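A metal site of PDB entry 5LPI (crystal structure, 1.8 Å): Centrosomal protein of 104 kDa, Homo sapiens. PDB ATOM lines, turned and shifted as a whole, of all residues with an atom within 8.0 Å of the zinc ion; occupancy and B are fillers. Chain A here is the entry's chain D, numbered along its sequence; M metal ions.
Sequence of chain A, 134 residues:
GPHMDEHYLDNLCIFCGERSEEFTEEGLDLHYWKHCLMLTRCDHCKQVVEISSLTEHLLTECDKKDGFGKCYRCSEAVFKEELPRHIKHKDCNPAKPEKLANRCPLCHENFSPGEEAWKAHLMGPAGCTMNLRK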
ATOM      1  N   LYS A  70       1.136  12.745  30.519  1.00  0.00           N
ATOM      2  CA  LYS A  70       0.242  13.847  30.214  1.00  0.00           C
ATOM      3  C   LYS A  70       1.049  15.033  29.706  1.00  0.00           C
ATOM      4  O   LYS A  70       1.995  15.475  30.372  1.00  0.00           O
ATOM      5  CB  LYS A  70      -0.566  14.255  31.450  1.00  0.00           C
ATOM      6  CG  LYS A  70      -1.476  15.453  31.225  1.00  0.00           C
ATOM      7  CD  LYS A  70      -2.364  15.676  32.434  1.00  0.00           C
ATOM      8  CE  LYS A  70      -3.407  16.734  32.189  1.00  0.00           C
ATOM      9  NZ  LYS A  70      -4.091  17.140  33.451  1.00  0.00           N
ATOM     10  N   CYS A  71       0.702  15.532  28.530  1.00  0.00           N
ATOM     11  CA  CYS A  71       1.288  16.788  28.097  1.00  0.00           C
ATOM     12  C   CYS A  71       0.625  17.931  28.844  1.00  0.00           C
ATOM     13  O   CYS A  71      -0.599  18.116  28.743  1.00  0.00           O
ATOM     14  CB  CYS A  71       1.149  16.995  26.587  1.00  0.00           C
ATOM     15  SG  CYS A  71       1.618  18.716  26.138  1.00  0.00           S
ATOM     16  N   TYR A  72       1.422  18.688  29.602  1.00  0.00           N
ATOM     17  CA  TYR A  72       0.873  19.799  30.354  1.00  0.00           C
ATOM     18  C   TYR A  72       0.365  20.926  29.463  1.00  0.00           C
ATOM     19  O   TYR A  72      -0.365  21.794  29.950  1.00  0.00           O
ATOM     20  CB  TYR A  72       1.929  20.315  31.344  1.00  0.00           C
ATOM     21  CG  TYR A  72       2.340  19.285  32.373  1.00  0.00           C
ATOM     22  CD1 TYR A  72       1.511  18.207  32.692  1.00  0.00           C
ATOM     23  CD2 TYR A  72       3.563  19.376  33.029  1.00  0.00           C
ATOM     24  CE1 TYR A  72       1.891  17.260  33.629  1.00  0.00           C
ATOM     25  CE2 TYR A  72       3.946  18.439  33.980  1.00  0.00           C
ATOM     26  CZ  TYR A  72       3.113  17.382  34.264  1.00  0.00           C
ATOM     27  OH  TYR A  72       3.501  16.445  35.206  1.00  0.00           O
ATOM     28  N   ARG A  73       0.713  20.918  28.169  1.00  0.00           N
ATOM     29  CA  ARG A  73       0.188  21.933  27.259  1.00  0.00           C
ATOM     30  C   ARG A  73      -1.225  21.599  26.807  1.00  0.00           C
ATOM     31  O   ARG A  73      -2.155  22.385  27.009  1.00  0.00           O
ATOM     32  CB  ARG A  73       1.124  22.106  26.054  1.00  0.00           C
ATOM     33  CG  ARG A  73       0.747  23.225  25.077  1.00  0.00           C
ATOM     34  CD  ARG A  73       1.784  23.311  23.946  1.00  0.00           C
ATOM     35  NE  ARG A  73       1.237  23.750  22.660  1.00  0.00           N
ATOM     36  CZ  ARG A  73       1.309  24.990  22.196  1.00  0.00           C
ATOM     37  NH1 ARG A  73       1.912  25.926  22.914  1.00  0.00           N
ATOM     38  NH2 ARG A  73       0.801  25.296  21.014  1.00  0.00           N
ATOM     39  N   CYS A  74      -1.413  20.417  26.214  1.00  0.00           N
ATOM     40  CA  CYS A  74      -2.720  20.064  25.683  1.00  0.00           C
ATOM     41  C   CYS A  74      -3.559  19.198  26.617  1.00  0.00           C
ATOM     42  O   CYS A  74      -4.727  18.965  26.316  1.00  0.00           O
ATOM     43  CB  CYS A  74      -2.574  19.331  24.337  1.00  0.00           C
ATOM     44  SG  CYS A  74      -1.633  17.810  24.436  1.00  0.00           S
ATOM     45  N   SER A  75      -2.989  18.719  27.727  1.00  0.00           N
ATOM     46  CA  SER A  75      -3.651  17.893  28.733  1.00  0.00           C
ATOM     47  C   SER A  75      -3.915  16.470  28.248  1.00  0.00           C
ATOM     48  O   SER A  75      -4.517  15.680  28.990  1.00  0.00           O
ATOM     49  CB  SER A  75      -4.981  18.486  29.220  1.00  0.00           C
ATOM     50  OG  SER A  75      -6.006  18.283  28.251  1.00  0.00           O
ATOM     51  N   GLU A  76      -3.489  16.103  27.049  1.00  0.00           N
ATOM     52  CA  GLU A  76      -3.748  14.783  26.507  1.00  0.00           C
ATOM     53  C   GLU A  76      -2.661  13.791  26.910  1.00  0.00           C
ATOM     54  O   GLU A  76      -1.555  14.165  27.327  1.00  0.00           O
ATOM     55  CB  GLU A  76      -3.858  14.852  24.979  1.00  0.00           C
ATOM     56  CG  GLU A  76      -5.030  15.731  24.494  1.00  0.00           C
ATOM     57  CD  GLU A  76      -5.183  15.757  22.983  1.00  0.00           C
ATOM     58  OE1 GLU A  76      -4.481  14.986  22.279  1.00  0.00           O
ATOM     59  OE2 GLU A  76      -5.999  16.562  22.489  1.00  0.00           O
ATOM     60  N   ALA A  77      -3.005  12.515  26.809  1.00  0.00           N
ATOM     61  CA  ALA A  77      -2.034  11.444  27.000  1.00  0.00           C
ATOM     62  C   ALA A  77      -1.191  11.260  25.745  1.00  0.00           C
ATOM     63  O   ALA A  77      -1.716  11.252  24.619  1.00  0.00           O
ATOM     64  CB  ALA A  77      -2.744  10.123  27.332  1.00  0.00           C
ATOM     65  N   VAL A  78       0.106  11.106  25.937  1.00  0.00           N
ATOM     66  CA  VAL A  78       1.062  10.862  24.870  1.00  0.00           C
ATOM     67  C   VAL A  78       1.922   9.692  25.300  1.00  0.00           C
ATOM     68  O   VAL A  78       2.207   9.540  26.494  1.00  0.00           O
ATOM     69  CB  VAL A  78       1.929  12.122  24.611  1.00  0.00           C
ATOM     70  CG1 VAL A  78       2.961  11.855  23.517  1.00  0.00           C
ATOM     71  CG2 VAL A  78       1.041  13.317  24.248  1.00  0.00           C
ATOM     72  N   LEU A  83       6.859  11.877  24.497  1.00  0.00           N
ATOM     73  CA  LEU A  83       6.446  13.100  25.187  1.00  0.00           C
ATOM     74  C   LEU A  83       7.501  14.202  25.174  1.00  0.00           C
ATOM     75  O   LEU A  83       7.113  15.367  24.969  1.00  0.00           O
ATOM     76  CB  LEU A  83       6.029  12.745  26.629  1.00  0.00           C
ATOM     77  CG  LEU A  83       5.386  13.824  27.486  1.00  0.00           C
ATOM     78  CD1 LEU A  83       4.223  14.534  26.760  1.00  0.00           C
ATOM     79  CD2 LEU A  83       4.882  13.227  28.799  1.00  0.00           C
ATOM     80  N   HIS A  86       7.197  15.567  21.723  1.00  0.00           N
ATOM     81  CA  HIS A  86       5.886  16.225  21.694  1.00  0.00           C
ATOM     82  C   HIS A  86       5.967  17.597  22.358  1.00  0.00           C
ATOM     83  O   HIS A  86       5.514  18.602  21.801  1.00  0.00           O
ATOM     84  CB  HIS A  86       4.826  15.354  22.373  1.00  0.00           C
ATOM     85  CG  HIS A  86       3.458  15.974  22.424  1.00  0.00           C
ATOM     86  ND1 HIS A  86       2.452  15.618  21.557  1.00  0.00           N
ATOM     87  CD2 HIS A  86       2.930  16.934  23.233  1.00  0.00           C
ATOM     88  CE1 HIS A  86       1.360  16.329  21.822  1.00  0.00           C
ATOM     89  NE2 HIS A  86       1.634  17.137  22.837  1.00  0.00           N
ATOM     90  N   ILE A  87       6.552  17.647  23.557  1.00  0.00           N
ATOM     91  CA  ILE A  87       6.664  18.897  24.298  1.00  0.00           C
ATOM     92  C   ILE A  87       7.562  19.878  23.570  1.00  0.00           C
ATOM     93  O   ILE A  87       7.254  21.074  23.484  1.00  0.00           O
ATOM     94  CB  ILE A  87       7.178  18.600  25.727  1.00  0.00           C
ATOM     95  CG1 ILE A  87       6.044  17.998  26.572  1.00  0.00           C
ATOM     96  CG2 ILE A  87       7.764  19.839  26.370  1.00  0.00           C
ATOM     97  CD1 ILE A  87       6.530  17.345  27.839  1.00  0.00           C
ATOM     98  N   LYS A  90       5.864  21.619  20.435  1.00  0.00           N
ATOM     99  CA  LYS A  90       4.854  22.634  20.774  1.00  0.00           C
ATOM    100  C   LYS A  90       3.807  22.806  19.674  1.00  0.00           C
ATOM    101  O   LYS A  90       3.372  23.912  19.356  1.00  0.00           O
ATOM    102  CB  LYS A  90       5.517  23.984  21.077  1.00  0.00           C
ATOM    103  CG  LYS A  90       6.255  24.050  22.389  1.00  0.00           C
ATOM    104  CD  LYS A  90       6.883  25.412  22.592  1.00  0.00           C
ATOM    105  CE  LYS A  90       7.963  25.373  23.664  1.00  0.00           C
ATOM    106  NZ  LYS A  90       8.630  26.698  23.863  1.00  0.00           N
ATOM    107  N   ASP A  91       3.390  21.688  19.069  1.00  0.00           N
ATOM    108  CA  ASP A  91       2.413  21.745  17.977  1.00  0.00           C
ATOM    109  C   ASP A  91       1.005  21.382  18.418  1.00  0.00           C
ATOM    110  O   ASP A  91       0.075  21.529  17.615  1.00  0.00           O
ATOM    111  CB  ASP A  91       2.847  20.834  16.829  1.00  0.00           C
ATOM    112  CG  ASP A  91       4.078  21.337  16.124  1.00  0.00           C
ATOM    113  OD1 ASP A  91       4.248  22.579  16.029  1.00  0.00           O
ATOM    114  OD2 ASP A  91       4.877  20.493  15.656  1.00  0.00           O
ATOM    115  N   CYS A  92       0.821  20.902  19.648  1.00  0.00           N
ATOM    116  CA  CYS A  92      -0.505  20.503  20.109  1.00  0.00           C
ATOM    117  C   CYS A  92      -1.349  21.732  20.424  1.00  0.00           C
ATOM    118  O   CYS A  92      -0.843  22.834  20.638  1.00  0.00           O
ATOM    119  CB  CYS A  92      -0.373  19.605  21.348  1.00  0.00           C
ATOM    120  SG  CYS A  92       0.504  20.391  22.722  1.00  0.00           S
ATOM    121  N   ASN A  93      -2.665  21.525  20.433  1.00  0.00           N
ATOM    122  CA  ASN A  93      -3.593  22.617  20.744  1.00  0.00           C
ATOM    123  C   ASN A  93      -3.679  22.805  22.251  1.00  0.00           C
ATOM    124  O   ASN A  93      -4.072  21.871  22.962  1.00  0.00           O
ATOM    125  CB  ASN A  93      -4.963  22.322  20.158  1.00  0.00           C
ATOM    126  CG  ASN A  93      -5.969  23.460  20.440  1.00  0.00           C
ATOM    127  OD1 ASN A  93      -5.583  24.599  20.739  1.00  0.00           O
ATOM    128  ND2 ASN A  93      -7.253  23.138  20.365  1.00  0.00           N
ATOM    129  N   PRO A  94      -3.361  23.989  22.781  1.00  0.00           N
ATOM    130  CA  PRO A  94      -3.363  24.165  24.243  1.00  0.00           C
ATOM    131  C   PRO A  94      -4.745  23.916  24.847  1.00  0.00           C
ATOM    132  O   PRO A  94      -5.782  24.149  24.222  1.00  0.00           O
ATOM    133  CB  PRO A  94      -2.924  25.614  24.425  1.00  0.00           C
ATOM    134  CG  PRO A  94      -2.135  25.928  23.182  1.00  0.00           C
ATOM    135  CD  PRO A  94      -2.839  25.182  22.085  1.00  0.00           C
ATOM    136  N   ALA A  95      -4.734  23.411  26.083  1.00  0.00           N
ATOM    137  CA  ALA A  95      -5.958  23.109  26.798  1.00  0.00           C
ATOM    138  C   ALA A  95      -6.422  24.324  27.596  1.00  0.00           C
ATOM    139  O   ALA A  95      -5.659  25.262  27.840  1.00  0.00           O
ATOM    140  CB  ALA A  95      -5.765  21.908  27.720  1.00  0.00           C
ATOM    141  N   ARG A 103     -12.815  19.250  25.964  1.00  0.00           N
ATOM    142  CA  ARG A 103     -11.689  18.980  25.085  1.00  0.00           C
ATOM    143  C   ARG A 103     -11.893  17.619  24.433  1.00  0.00           C
ATOM    144  O   ARG A 103     -11.932  16.602  25.121  1.00  0.00           O
ATOM    145  CB  ARG A 103     -10.365  19.003  25.853  1.00  0.00           C
ATOM    146  CG  ARG A 103      -9.196  18.389  25.108  1.00  0.00           C
ATOM    147  CD  ARG A 103      -8.930  19.109  23.796  1.00  0.00           C
ATOM    148  NE  ARG A 103      -7.601  18.839  23.266  1.00  0.00           N
ATOM    149  CZ  ARG A 103      -6.630  19.748  23.153  1.00  0.00           C
ATOM    150  NH1 ARG A 103      -6.845  21.011  23.520  1.00  0.00           N
ATOM    151  NH2 ARG A 103      -5.454  19.406  22.633  1.00  0.00           N
HETATM  152 ZN    ZN M   1       0.594  18.496  23.976  1.00  0.00          ZN
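Within 4 Å of the zinc ion: Cys 71, Cys 74, His 86 and Cys 92.
The backbone carbonyl oxygen of Glu 76 is in hydrogen-bond range of the backbone NH of Cys 71 (2.9 Å). The backbone NH (N) of Glu 76 sits close to the side-chain sulfur (SG) of Cys 74, 3.6 Å away. The guanidinium group (NH2) of Arg 73 sits at hydrogen-bond distance from the backbone carbonyl oxygen (O) of Cys 92. The side-chain sulfur (SG) of Cys 71 lies close to the backbone NH (N) of Arg 73, 3.1 Å away.
The zinc ion is bound by a ring nitrogen (NE2) of His 86 (2.1 Å), the side-chain sulfur (SG) of Cys 92 (2.3 Å), the side-chain sulfur (SG) of Cys 74 (2.4 Å) and the side-chain sulfur (SG) of Cys 71 (2.4 Å).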
